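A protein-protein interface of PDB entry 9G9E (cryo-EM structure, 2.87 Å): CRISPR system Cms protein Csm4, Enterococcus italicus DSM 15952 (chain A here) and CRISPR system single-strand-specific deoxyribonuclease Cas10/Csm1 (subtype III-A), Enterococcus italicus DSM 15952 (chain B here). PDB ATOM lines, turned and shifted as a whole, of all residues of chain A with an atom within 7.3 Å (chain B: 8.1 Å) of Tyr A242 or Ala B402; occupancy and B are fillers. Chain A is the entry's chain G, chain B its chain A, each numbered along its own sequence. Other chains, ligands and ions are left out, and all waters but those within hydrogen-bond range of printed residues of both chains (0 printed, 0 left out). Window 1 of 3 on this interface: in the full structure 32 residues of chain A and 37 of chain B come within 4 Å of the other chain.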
ATOM      1  N   LEU A  77       8.046   3.662 -19.938  1.00  0.00           N
ATOM      2  CA  LEU A  77       9.088   4.642 -19.638  1.00  0.00           C
ATOM      3  C   LEU A  77       8.502   5.673 -18.680  1.00  0.00           C
ATOM      4  O   LEU A  77       8.286   6.838 -19.017  1.00  0.00           O
ATOM      5  CB  LEU A  77       9.612   5.279 -20.918  1.00  0.00           C
ATOM      6  CG  LEU A  77      10.276   4.327 -21.915  1.00  0.00           C
ATOM      7  CD1 LEU A  77      10.916   5.104 -23.051  1.00  0.00           C
ATOM      8  CD2 LEU A  77      11.297   3.439 -21.223  1.00  0.00           C
ATOM      9  N   LEU A 222       3.047   3.097 -25.689  1.00  0.00           N
ATOM     10  CA  LEU A 222       3.175   2.594 -27.050  1.00  0.00           C
ATOM     11  C   LEU A 222       3.456   1.098 -27.017  1.00  0.00           C
ATOM     12  O   LEU A 222       4.330   0.639 -26.277  1.00  0.00           O
ATOM     13  CB  LEU A 222       4.290   3.333 -27.787  1.00  0.00           C
ATOM     14  CG  LEU A 222       3.872   4.223 -28.955  1.00  0.00           C
ATOM     15  CD1 LEU A 222       5.096   4.725 -29.700  1.00  0.00           C
ATOM     16  CD2 LEU A 222       2.944   3.470 -29.888  1.00  0.00           C
ATOM     17  N   MET A 227       5.392   6.704 -34.870  1.00  0.00           N
ATOM     18  CA  MET A 227       5.681   8.128 -34.941  1.00  0.00           C
ATOM     19  C   MET A 227       4.502   8.814 -35.608  1.00  0.00           C
ATOM     20  O   MET A 227       3.877   8.257 -36.515  1.00  0.00           O
ATOM     21  CB  MET A 227       6.983   8.409 -35.703  1.00  0.00           C
ATOM     22  CG  MET A 227       7.368   9.882 -35.768  1.00  0.00           C
ATOM     23  SD  MET A 227       8.114  10.521 -34.257  1.00  0.00           S
ATOM     24  CE  MET A 227       9.592   9.532 -34.150  1.00  0.00           C
ATOM     25  N   CYS A 236       1.611  16.312 -29.168  1.00  0.00           N
ATOM     26  CA  CYS A 236       1.697  15.028 -28.482  1.00  0.00           C
ATOM     27  C   CYS A 236       3.014  14.817 -27.744  1.00  0.00           C
ATOM     28  O   CYS A 236       3.169  13.790 -27.076  1.00  0.00           O
ATOM     29  CB  CYS A 236       1.491  13.881 -29.477  1.00  0.00           C
ATOM     30  SG  CYS A 236       2.959  13.455 -30.440  1.00  0.00           S
ATOM     31  N   LEU A 237       3.959  15.750 -27.844  1.00  0.00           N
ATOM     32  CA  LEU A 237       5.293  15.564 -27.290  1.00  0.00           C
ATOM     33  C   LEU A 237       5.484  16.214 -25.925  1.00  0.00           C
ATOM     34  O   LEU A 237       6.594  16.170 -25.388  1.00  0.00           O
ATOM     35  CB  LEU A 237       6.343  16.103 -28.266  1.00  0.00           C
ATOM     36  CG  LEU A 237       7.625  15.280 -28.399  1.00  0.00           C
ATOM     37  CD1 LEU A 237       7.301  13.804 -28.565  1.00  0.00           C
ATOM     38  CD2 LEU A 237       8.459  15.780 -29.565  1.00  0.00           C
ATOM     39  N   ASP A 239       5.541  16.579 -22.022  1.00  0.00           N
ATOM     40  CA  ASP A 239       5.664  15.704 -20.853  1.00  0.00           C
ATOM     41  C   ASP A 239       5.833  14.240 -21.252  1.00  0.00           C
ATOM     42  O   ASP A 239       5.477  13.334 -20.495  1.00  0.00           O
ATOM     43  CB  ASP A 239       4.471  15.864 -19.906  1.00  0.00           C
ATOM     44  CG  ASP A 239       4.564  17.115 -19.055  1.00  0.00           C
ATOM     45  OD1 ASP A 239       4.417  18.225 -19.607  1.00  0.00           O
ATOM     46  OD2 ASP A 239       4.784  16.987 -17.832  1.00  0.00           O
ATOM     47  N   ALA A 240       6.379  13.997 -22.438  1.00  0.00           N
ATOM     48  CA  ALA A 240       6.561  12.645 -22.941  1.00  0.00           C
ATOM     49  C   ALA A 240       7.897  12.069 -22.490  1.00  0.00           C
ATOM     50  O   ALA A 240       8.880  12.792 -22.303  1.00  0.00           O
ATOM     51  CB  ALA A 240       6.475  12.621 -24.468  1.00  0.00           C
ATOM     52  N   ARG A 241       7.920  10.752 -22.312  1.00  0.00           N
ATOM     53  CA  ARG A 241       9.130  10.004 -21.977  1.00  0.00           C
ATOM     54  C   ARG A 241       9.260   8.885 -23.004  1.00  0.00           C
ATOM     55  O   ARG A 241       8.559   7.872 -22.919  1.00  0.00           O
ATOM     56  CB  ARG A 241       9.067   9.458 -20.555  1.00  0.00           C
ATOM     57  CG  ARG A 241       8.853  10.514 -19.486  1.00  0.00           C
ATOM     58  CD  ARG A 241       8.877   9.898 -18.097  1.00  0.00           C
ATOM     59  NE  ARG A 241      10.140   9.226 -17.812  1.00  0.00           N
ATOM     60  CZ  ARG A 241      11.125   9.755 -17.102  1.00  0.00           C
ATOM     61  NH1 ARG A 241      11.031  10.969 -16.587  1.00  0.00           N
ATOM     62  NH2 ARG A 241      12.232   9.046 -16.900  1.00  0.00           N
ATOM     63  N   TYR A 242      10.157   9.064 -23.971  1.00  0.00           N
ATOM     64  CA  TYR A 242      10.240   8.144 -25.099  1.00  0.00           C
ATOM     65  C   TYR A 242      11.671   7.692 -25.361  1.00  0.00           C
ATOM     66  O   TYR A 242      12.576   7.963 -24.565  1.00  0.00           O
ATOM     67  CB  TYR A 242       9.657   8.803 -26.351  1.00  0.00           C
ATOM     68  CG  TYR A 242      10.361  10.078 -26.754  1.00  0.00           C
ATOM     69  CD1 TYR A 242      11.509  10.044 -27.536  1.00  0.00           C
ATOM     70  CD2 TYR A 242       9.887  11.315 -26.342  1.00  0.00           C
ATOM     71  CE1 TYR A 242      12.156  11.202 -27.900  1.00  0.00           C
ATOM     72  CE2 TYR A 242      10.530  12.480 -26.703  1.00  0.00           C
ATOM     73  CZ  TYR A 242      11.664  12.415 -27.483  1.00  0.00           C
ATOM     74  OH  TYR A 242      12.312  13.568 -27.848  1.00  0.00           O
ATOM     75  N   LEU A 243      11.877   6.996 -26.477  1.00  0.00           N
ATOM     76  CA  LEU A 243      13.207   6.570 -26.897  1.00  0.00           C
ATOM     77  C   LEU A 243      13.224   6.485 -28.414  1.00  0.00           C
ATOM     78  O   LEU A 243      12.502   5.670 -28.996  1.00  0.00           O
ATOM     79  CB  LEU A 243      13.581   5.222 -26.279  1.00  0.00           C
ATOM     80  CG  LEU A 243      14.979   4.709 -26.625  1.00  0.00           C
ATOM     81  CD1 LEU A 243      16.037   5.479 -25.852  1.00  0.00           C
ATOM     82  CD2 LEU A 243      15.091   3.218 -26.356  1.00  0.00           C
ATOM     83  N   LEU A 244      14.036   7.324 -29.051  1.00  0.00           N
ATOM     84  CA  LEU A 244      14.131   7.330 -30.505  1.00  0.00           C
ATOM     85  C   LEU A 244      15.004   6.179 -30.984  1.00  0.00           C
ATOM     86  O   LEU A 244      16.134   6.006 -30.518  1.00  0.00           O
ATOM     87  CB  LEU A 244      14.698   8.661 -30.997  1.00  0.00           C
ATOM     88  CG  LEU A 244      13.689   9.761 -31.322  1.00  0.00           C
ATOM     89  CD1 LEU A 244      14.344  10.859 -32.142  1.00  0.00           C
ATOM     90  CD2 LEU A 244      12.496   9.186 -32.055  1.00  0.00           C
ATOM     91  N   LYS A 245      14.479   5.394 -31.921  1.00  0.00           N
ATOM     92  CA  LYS A 245      15.207   4.310 -32.555  1.00  0.00           C
ATOM     93  C   LYS A 245      15.407   4.629 -34.027  1.00  0.00           C
ATOM     94  O   LYS A 245      14.479   5.085 -34.706  1.00  0.00           O
ATOM     95  CB  LYS A 245      14.465   2.979 -32.408  1.00  0.00           C
ATOM     96  CG  LYS A 245      14.619   2.320 -31.049  1.00  0.00           C
ATOM     97  CD  LYS A 245      16.044   2.412 -30.531  1.00  0.00           C
ATOM     98  CE  LYS A 245      16.297   1.383 -29.443  1.00  0.00           C
ATOM     99  NZ  LYS A 245      17.269   0.340 -29.873  1.00  0.00           N
ATOM    100  N   ALA A 268      11.852   6.370 -35.125  1.00  0.00           N
ATOM    101  CA  ALA A 268      10.553   6.033 -34.558  1.00  0.00           C
ATOM    102  C   ALA A 268      10.642   5.939 -33.042  1.00  0.00           C
ATOM    103  O   ALA A 268      11.673   5.558 -32.487  1.00  0.00           O
ATOM    104  CB  ALA A 268      10.017   4.712 -35.127  1.00  0.00           C
ATOM    105  N   PHE A 269       9.548   6.297 -32.373  1.00  0.00           N
ATOM    106  CA  PHE A 269       9.466   6.101 -30.932  1.00  0.00           C
ATOM    107  C   PHE A 269       9.451   4.614 -30.606  1.00  0.00           C
ATOM    108  O   PHE A 269       8.909   3.802 -31.359  1.00  0.00           O
ATOM    109  CB  PHE A 269       8.218   6.778 -30.365  1.00  0.00           C
ATOM    110  CG  PHE A 269       8.231   8.274 -30.480  1.00  0.00           C
ATOM    111  CD1 PHE A 269       9.361   8.999 -30.142  1.00  0.00           C
ATOM    112  CD2 PHE A 269       7.108   8.958 -30.911  1.00  0.00           C
ATOM    113  CE1 PHE A 269       9.373  10.376 -30.243  1.00  0.00           C
ATOM    114  CE2 PHE A 269       7.114  10.335 -31.010  1.00  0.00           C
ATOM    115  CZ  PHE A 269       8.249  11.044 -30.678  1.00  0.00           C
ATOM    116  N   SER A 270      10.050   4.259 -29.473  1.00  0.00           N
ATOM    117  CA  SER A 270      10.170   2.863 -29.088  1.00  0.00           C
ATOM    118  C   SER A 270       8.865   2.349 -28.484  1.00  0.00           C
ATOM    119  O   SER A 270       7.933   3.105 -28.195  1.00  0.00           O
ATOM    120  CB  SER A 270      11.309   2.678 -28.088  1.00  0.00           C
ATOM    121  OG  SER A 270      12.516   2.340 -28.743  1.00  0.00           O
ATOM    122  N   GLY A 272       6.891   1.086 -25.370  1.00  0.00           N
ATOM    123  CA  GLY A 272       6.981   1.455 -23.976  1.00  0.00           C
ATOM    124  C   GLY A 272       7.002   2.946 -23.723  1.00  0.00           C
ATOM    125  O   GLY A 272       6.856   3.362 -22.568  1.00  0.00           O
ATOM    126  N   SER A 273       7.179   3.757 -24.764  1.00  0.00           N
ATOM    127  CA  SER A 273       7.184   5.204 -24.603  1.00  0.00           C
ATOM    128  C   SER A 273       5.832   5.687 -24.097  1.00  0.00           C
ATOM    129  O   SER A 273       4.782   5.264 -24.587  1.00  0.00           O
ATOM    130  CB  SER A 273       7.524   5.877 -25.932  1.00  0.00           C
ATOM    131  OG  SER A 273       8.679   5.299 -26.513  1.00  0.00           O
ATOM    132  N   THR A 274       5.860   6.581 -23.113  1.00  0.00           N
ATOM    133  CA  THR A 274       4.649   7.072 -22.470  1.00  0.00           C
ATOM    134  C   THR A 274       4.345   8.486 -22.943  1.00  0.00           C
ATOM    135  O   THR A 274       5.214   9.363 -22.897  1.00  0.00           O
ATOM    136  CB  THR A 274       4.788   7.050 -20.948  1.00  0.00           C
ATOM    137  OG1 THR A 274       6.106   7.474 -20.582  1.00  0.00           O
ATOM    138  CG2 THR A 274       4.547   5.647 -20.413  1.00  0.00           C
ATOM    139  N   PHE A 275       3.113   8.700 -23.394  1.00  0.00           N
ATOM    140  CA  PHE A 275       2.644  10.004 -23.831  1.00  0.00           C
ATOM    141  C   PHE A 275       1.345  10.336 -23.114  1.00  0.00           C
ATOM    142  O   PHE A 275       0.547   9.450 -22.799  1.00  0.00           O
ATOM    143  CB  PHE A 275       2.413  10.051 -25.351  1.00  0.00           C
ATOM    144  CG  PHE A 275       3.647   9.783 -26.165  1.00  0.00           C
ATOM    145  CD1 PHE A 275       4.085   8.488 -26.380  1.00  0.00           C
ATOM    146  CD2 PHE A 275       4.363  10.828 -26.722  1.00  0.00           C
ATOM    147  CE1 PHE A 275       5.217   8.242 -27.129  1.00  0.00           C
ATOM    148  CE2 PHE A 275       5.496  10.587 -27.471  1.00  0.00           C
ATOM    149  CZ  PHE A 275       5.923   9.292 -27.675  1.00  0.00           C
ATOM    150  N   SER B 277      25.387   9.991 -23.775  1.00  0.00           N
ATOM    151  CA  SER B 277      24.586   8.836 -24.149  1.00  0.00           C
ATOM    152  C   SER B 277      24.971   8.384 -25.550  1.00  0.00           C
ATOM    153  O   SER B 277      25.206   9.213 -26.438  1.00  0.00           O
ATOM    154  CB  SER B 277      23.089   9.158 -24.093  1.00  0.00           C
ATOM    155  OG  SER B 277      22.769   9.901 -22.930  1.00  0.00           O
ATOM    156  N   ALA B 368      23.322  15.195 -21.979  1.00  0.00           N
ATOM    157  CA  ALA B 368      22.247  15.704 -21.143  1.00  0.00           C
ATOM    158  C   ALA B 368      22.832  16.429 -19.940  1.00  0.00           C
ATOM    159  O   ALA B 368      23.752  15.925 -19.287  1.00  0.00           O
ATOM    160  CB  ALA B 368      21.328  14.573 -20.676  1.00  0.00           C
ATOM    161  N   ARG B 395      18.135  12.214 -10.634  1.00  0.00           N
ATOM    162  CA  ARG B 395      16.787  12.012 -11.158  1.00  0.00           C
ATOM    163  C   ARG B 395      16.449  13.037 -12.235  1.00  0.00           C
ATOM    164  O   ARG B 395      15.810  12.703 -13.239  1.00  0.00           O
ATOM    165  CB  ARG B 395      15.767  12.065 -10.022  1.00  0.00           C
ATOM    166  CG  ARG B 395      15.730  10.808  -9.162  1.00  0.00           C
ATOM    167  CD  ARG B 395      15.614   9.549 -10.011  1.00  0.00           C
ATOM    168  NE  ARG B 395      16.906   8.906 -10.217  1.00  0.00           N
ATOM    169  CZ  ARG B 395      17.180   8.075 -11.213  1.00  0.00           C
ATOM    170  NH1 ARG B 395      16.270   7.756 -12.119  1.00  0.00           N
ATOM    171  NH2 ARG B 395      18.399   7.551 -11.305  1.00  0.00           N
ATOM    172  N   LYS B 396      16.868  14.289 -12.048  1.00  0.00           N
ATOM    173  CA  LYS B 396      16.664  15.295 -13.085  1.00  0.00           C
ATOM    174  C   LYS B 396      17.459  14.957 -14.338  1.00  0.00           C
ATOM    175  O   LYS B 396      16.991  15.181 -15.459  1.00  0.00           O
ATOM    176  CB  LYS B 396      17.041  16.680 -12.558  1.00  0.00           C
ATOM    177  CG  LYS B 396      16.097  17.208 -11.490  1.00  0.00           C
ATOM    178  CD  LYS B 396      16.606  18.506 -10.887  1.00  0.00           C
ATOM    179  CE  LYS B 396      16.631  19.621 -11.917  1.00  0.00           C
ATOM    180  NZ  LYS B 396      15.274  19.910 -12.459  1.00  0.00           N
ATOM    181  N   LEU B 397      18.667  14.413 -14.168  1.00  0.00           N
ATOM    182  CA  LEU B 397      19.452  13.978 -15.319  1.00  0.00           C
ATOM    183  C   LEU B 397      18.754  12.853 -16.072  1.00  0.00           C
ATOM    184  O   LEU B 397      18.730  12.844 -17.309  1.00  0.00           O
ATOM    185  CB  LEU B 397      20.843  13.537 -14.865  1.00  0.00           C
ATOM    186  CG  LEU B 397      21.842  13.192 -15.968  1.00  0.00           C
ATOM    187  CD1 LEU B 397      22.229  14.436 -16.747  1.00  0.00           C
ATOM    188  CD2 LEU B 397      23.066  12.518 -15.378  1.00  0.00           C
ATOM    189  N   SER B 398      18.184  11.891 -15.346  1.00  0.00           N
ATOM    190  CA  SER B 398      17.464  10.804 -16.005  1.00  0.00           C
ATOM    191  C   SER B 398      16.213  11.320 -16.709  1.00  0.00           C
ATOM    192  O   SER B 398      15.867  10.853 -17.801  1.00  0.00           O
ATOM    193  CB  SER B 398      17.106   9.714 -14.994  1.00  0.00           C
ATOM    194  OG  SER B 398      16.060  10.125 -14.136  1.00  0.00           O
ATOM    195  N   ASP B 399      15.524  12.288 -16.099  1.00  0.00           N
ATOM    196  CA  ASP B 399      14.373  12.903 -16.753  1.00  0.00           C
ATOM    197  C   ASP B 399      14.787  13.621 -18.032  1.00  0.00           C
ATOM    198  O   ASP B 399      14.076  13.569 -19.043  1.00  0.00           O
ATOM    199  CB  ASP B 399      13.678  13.871 -15.797  1.00  0.00           C
ATOM    200  CG  ASP B 399      12.956  13.161 -14.669  1.00  0.00           C
ATOM    201  OD1 ASP B 399      13.019  11.916 -14.609  1.00  0.00           O
ATOM    202  OD2 ASP B 399      12.325  13.851 -13.840  1.00  0.00           O
ATOM    203  N   LYS B 400      15.932  14.308 -18.001  1.00  0.00           N
ATOM    204  CA  LYS B 400      16.454  14.945 -19.205  1.00  0.00           C
ATOM    205  C   LYS B 400      16.776  13.912 -20.276  1.00  0.00           C
ATOM    206  O   LYS B 400      16.489  14.122 -21.460  1.00  0.00           O
ATOM    207  CB  LYS B 400      17.700  15.763 -18.866  1.00  0.00           C
ATOM    208  CG  LYS B 400      17.543  17.263 -19.033  1.00  0.00           C
ATOM    209  CD  LYS B 400      16.761  17.871 -17.884  1.00  0.00           C
ATOM    210  CE  LYS B 400      16.433  19.327 -18.157  1.00  0.00           C
ATOM    211  NZ  LYS B 400      17.658  20.118 -18.461  1.00  0.00           N
ATOM    212  N   LYS B 401      17.377  12.790 -19.878  1.00  0.00           N
ATOM    213  CA  LYS B 401      17.702  11.733 -20.827  1.00  0.00           C
ATOM    214  C   LYS B 401      16.461  11.022 -21.351  1.00  0.00           C
ATOM    215  O   LYS B 401      16.536  10.364 -22.394  1.00  0.00           O
ATOM    216  CB  LYS B 401      18.650  10.720 -20.185  1.00  0.00           C
ATOM    217  CG  LYS B 401      20.016  11.287 -19.840  1.00  0.00           C
ATOM    218  CD  LYS B 401      21.008  10.190 -19.501  1.00  0.00           C
ATOM    219  CE  LYS B 401      20.694   9.561 -18.155  1.00  0.00           C
ATOM    220  NZ  LYS B 401      21.778   8.649 -17.703  1.00  0.00           N
ATOM    221  N   ALA B 402      15.328  11.136 -20.658  1.00  0.00           N
ATOM    222  CA  ALA B 402      14.092  10.537 -21.150  1.00  0.00           C
ATOM    223  C   ALA B 402      13.535  11.320 -22.336  1.00  0.00           C
ATOM    224  O   ALA B 402      13.384  10.779 -23.436  1.00  0.00           O
ATOM    225  CB  ALA B 402      13.060  10.457 -20.023  1.00  0.00           C
ATOM    226  N   HIS B 403      13.223  12.598 -22.126  1.00  0.00           N
ATOM    227  CA  HIS B 403      12.761  13.484 -23.196  1.00  0.00           C
ATOM    228  C   HIS B 403      13.985  14.206 -23.743  1.00  0.00           C
ATOM    229  O   HIS B 403      14.402  15.246 -23.233  1.00  0.00           O
ATOM    230  CB  HIS B 403      11.707  14.452 -22.674  1.00  0.00           C
ATOM    231  CG  HIS B 403      10.977  15.192 -23.751  1.00  0.00           C
ATOM    232  ND1 HIS B 403      11.605  16.057 -24.620  1.00  0.00           N
ATOM    233  CD2 HIS B 403       9.668  15.193 -24.098  1.00  0.00           C
ATOM    234  CE1 HIS B 403      10.715  16.562 -25.456  1.00  0.00           C
ATOM    235  NE2 HIS B 403       9.533  16.053 -25.161  1.00  0.00           N
ATOM    236  N   LYS B 404      14.567  13.646 -24.802  1.00  0.00           N
ATOM    237  CA  LYS B 404      15.877  14.072 -25.280  1.00  0.00           C
ATOM    238  C   LYS B 404      15.825  15.101 -26.400  1.00  0.00           C
ATOM    239  O   LYS B 404      16.713  15.956 -26.474  1.00  0.00           O
ATOM    240  CB  LYS B 404      16.676  12.853 -25.757  1.00  0.00           C
ATOM    241  CG  LYS B 404      18.172  13.083 -25.847  1.00  0.00           C
ATOM    242  CD  LYS B 404      18.935  12.014 -25.086  1.00  0.00           C
ATOM    243  CE  LYS B 404      18.596  10.624 -25.595  1.00  0.00           C
ATOM    244  NZ  LYS B 404      19.340   9.568 -24.857  1.00  0.00           N
ATOM    245  N   TYR B 405      14.821  15.050 -27.271  1.00  0.00           N
ATOM    246  CA  TYR B 405      14.763  15.911 -28.442  1.00  0.00           C
ATOM    247  C   TYR B 405      13.450  16.681 -28.476  1.00  0.00           C
ATOM    248  O   TYR B 405      12.454  16.272 -27.873  1.00  0.00           O
ATOM    249  CB  TYR B 405      14.918  15.100 -29.735  1.00  0.00           C
ATOM    250  CG  TYR B 405      16.113  14.174 -29.739  1.00  0.00           C
ATOM    251  CD1 TYR B 405      17.392  14.660 -29.971  1.00  0.00           C
ATOM    252  CD2 TYR B 405      15.961  12.813 -29.513  1.00  0.00           C
ATOM    253  CE1 TYR B 405      18.486  13.817 -29.976  1.00  0.00           C
ATOM    254  CE2 TYR B 405      17.050  11.962 -29.517  1.00  0.00           C
ATOM    255  CZ  TYR B 405      18.309  12.471 -29.748  1.00  0.00           C
ATOM    256  OH  TYR B 405      19.397  11.628 -29.752  1.00  0.00           O
ATOM    257  N   SER B 406      13.460  17.807 -29.183  1.00  0.00           N
ATOM    258  CA  SER B 406      12.257  18.597 -29.382  1.00  0.00           C
ATOM    259  C   SER B 406      11.533  18.127 -30.642  1.00  0.00           C
ATOM    260  O   SER B 406      12.020  17.276 -31.389  1.00  0.00           O
ATOM    261  CB  SER B 406      12.599  20.083 -29.459  1.00  0.00           C
ATOM    262  OG  SER B 406      13.426  20.361 -30.575  1.00  0.00           O
ATOM    263  N   LEU B 407      10.343  18.686 -30.879  1.00  0.00           N
ATOM    264  CA  LEU B 407       9.564  18.294 -32.048  1.00  0.00           C
ATOM    265  C   LEU B 407      10.277  18.669 -33.342  1.00  0.00           C
ATOM    266  O   LEU B 407      10.278  17.893 -34.305  1.00  0.00           O
ATOM    267  CB  LEU B 407       8.169  18.923 -31.993  1.00  0.00           C
ATOM    268  CG  LEU B 407       8.004  20.438 -32.153  1.00  0.00           C
ATOM    269  CD1 LEU B 407       6.602  20.769 -32.634  1.00  0.00           C
ATOM    270  CD2 LEU B 407       8.303  21.169 -30.852  1.00  0.00           C
ATOM    271  N   GLU B 409      13.504  18.934 -33.871  1.00  0.00           N
ATOM    272  CA  GLU B 409      14.642  18.047 -34.090  1.00  0.00           C
ATOM    273  C   GLU B 409      14.197  16.704 -34.654  1.00  0.00           C
ATOM    274  O   GLU B 409      14.828  16.172 -35.573  1.00  0.00           O
ATOM    275  CB  GLU B 409      15.415  17.864 -32.786  1.00  0.00           C
ATOM    276  CG  GLU B 409      15.932  19.169 -32.201  1.00  0.00           C
ATOM    277  CD  GLU B 409      16.626  18.984 -30.868  1.00  0.00           C
ATOM    278  OE1 GLU B 409      16.663  17.841 -30.369  1.00  0.00           O
ATOM    279  OE2 GLU B 409      17.136  19.983 -30.320  1.00  0.00           O
ATOM    280  N   ILE B 410      13.102  16.147 -34.134  1.00  0.00           N
ATOM    281  CA  ILE B 410      12.595  14.880 -34.655  1.00  0.00           C
ATOM    282  C   ILE B 410      12.093  15.047 -36.085  1.00  0.00           C
ATOM    283  O   ILE B 410      12.332  14.189 -36.948  1.00  0.00           O
ATOM    284  CB  ILE B 410      11.500  14.321 -33.729  1.00  0.00           C
ATOM    285  CG1 ILE B 410      12.042  14.149 -32.309  1.00  0.00           C
ATOM    286  CG2 ILE B 410      10.973  12.999 -34.261  1.00  0.00           C
ATOM    287  CD1 ILE B 410      11.005  13.688 -31.311  1.00  0.00           C
ATOM    288  N   PHE B 413      14.921  15.090 -38.230  1.00  0.00           N
ATOM    289  CA  PHE B 413      15.465  13.738 -38.297  1.00  0.00           C
ATOM    290  C   PHE B 413      14.754  12.915 -39.360  1.00  0.00           C
ATOM    291  O   PHE B 413      15.392  12.175 -40.116  1.00  0.00           O
ATOM    292  CB  PHE B 413      15.346  13.057 -36.933  1.00  0.00           C
ATOM    293  CG  PHE B 413      16.522  13.286 -36.032  1.00  0.00           C
ATOM    294  CD1 PHE B 413      17.801  13.388 -36.550  1.00  0.00           C
ATOM    295  CD2 PHE B 413      16.347  13.394 -34.663  1.00  0.00           C
ATOM    296  CE1 PHE B 413      18.882  13.598 -35.718  1.00  0.00           C
ATOM    297  CE2 PHE B 413      17.424  13.604 -33.828  1.00  0.00           C
ATOM    298  CZ  PHE B 413      18.694  13.705 -34.356  1.00  0.00           C
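OH of Tyr A242 sits at hydrogen-bond distance from O of Tyr B405, at 2.7 Å.
O of Ala B402 lies close to O of Tyr A242, 3.1 Å away.
The side-chain carboxylate of Asp B399 is in salt-bridge range of the guanidinium group of Arg A241 (3.0 Å).
O of Leu A237 is in hydrogen-bond range of NE2 of His B403 (3.0 Å).
Of the printed residues of chain B, Tyr A242 touches Ala B402, His B403, Lys B404, Tyr B405 and Ile B410.
Of chain A, only Arg A241 and Tyr A242 come within 4 Å of Ala B402.
Printed residues of chain B within 4 Å of Phe A269: Ile B410 (3.8 Å).
Printed residues of chain B within 4 Å of Leu A244: Tyr B405.
Of the printed residues of chain A, Asp B399 touches Arg A241 (3.0 Å).
Of the printed residues of chain B, Ala A240 touches His B403.
Lys B401 touches none of the printed residues of chain A.
Ser B277 touches none of the printed residues of chain A.
The nearest residue of chain B that does not touch Tyr A242 is Ser B406 (4.6 Å).
The nearest residue of chain A that does not touch Ala B402 is Ala A240 (4.9 Å).
Among the printed residues, pairs that only touch across the chains: Met A227 with Ile B410, Leu A237 with Leu B407, Leu A237 with Ile B410, Ala A240 with His B403, Arg A241 with Ala B402, Tyr A242 with His B403, Tyr A242 with Lys B404, Tyr A242 with Ile B410, Leu A244 with Tyr B405 and Phe A269 with Ile B410.
Of the 19 printed residues of chain A, 7 touch a printed residue of chain B.
Hydrophobic or aromatic side chains of chain A within 4 Å of the printed part of chain B: Met A227, Leu A237, Tyr A242, Leu A244 and Phe A269.
Among the printed residues, Asp or Glu carboxylates within 4 Å of a Lys or Arg side-chain nitrogen of the other chain: Arg A241 with Asp B399.
O of Tyr B405 sits close to ND1 of His B403 (3.4 Å).
O of Arg A241 is in hydrogen-bond range of N of Thr A274 (3.0 Å).
The guanidinium group (NE) of Arg A241 lies close to the backbone carbonyl oxygen (O) of Leu A77, at 3.3 Å.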
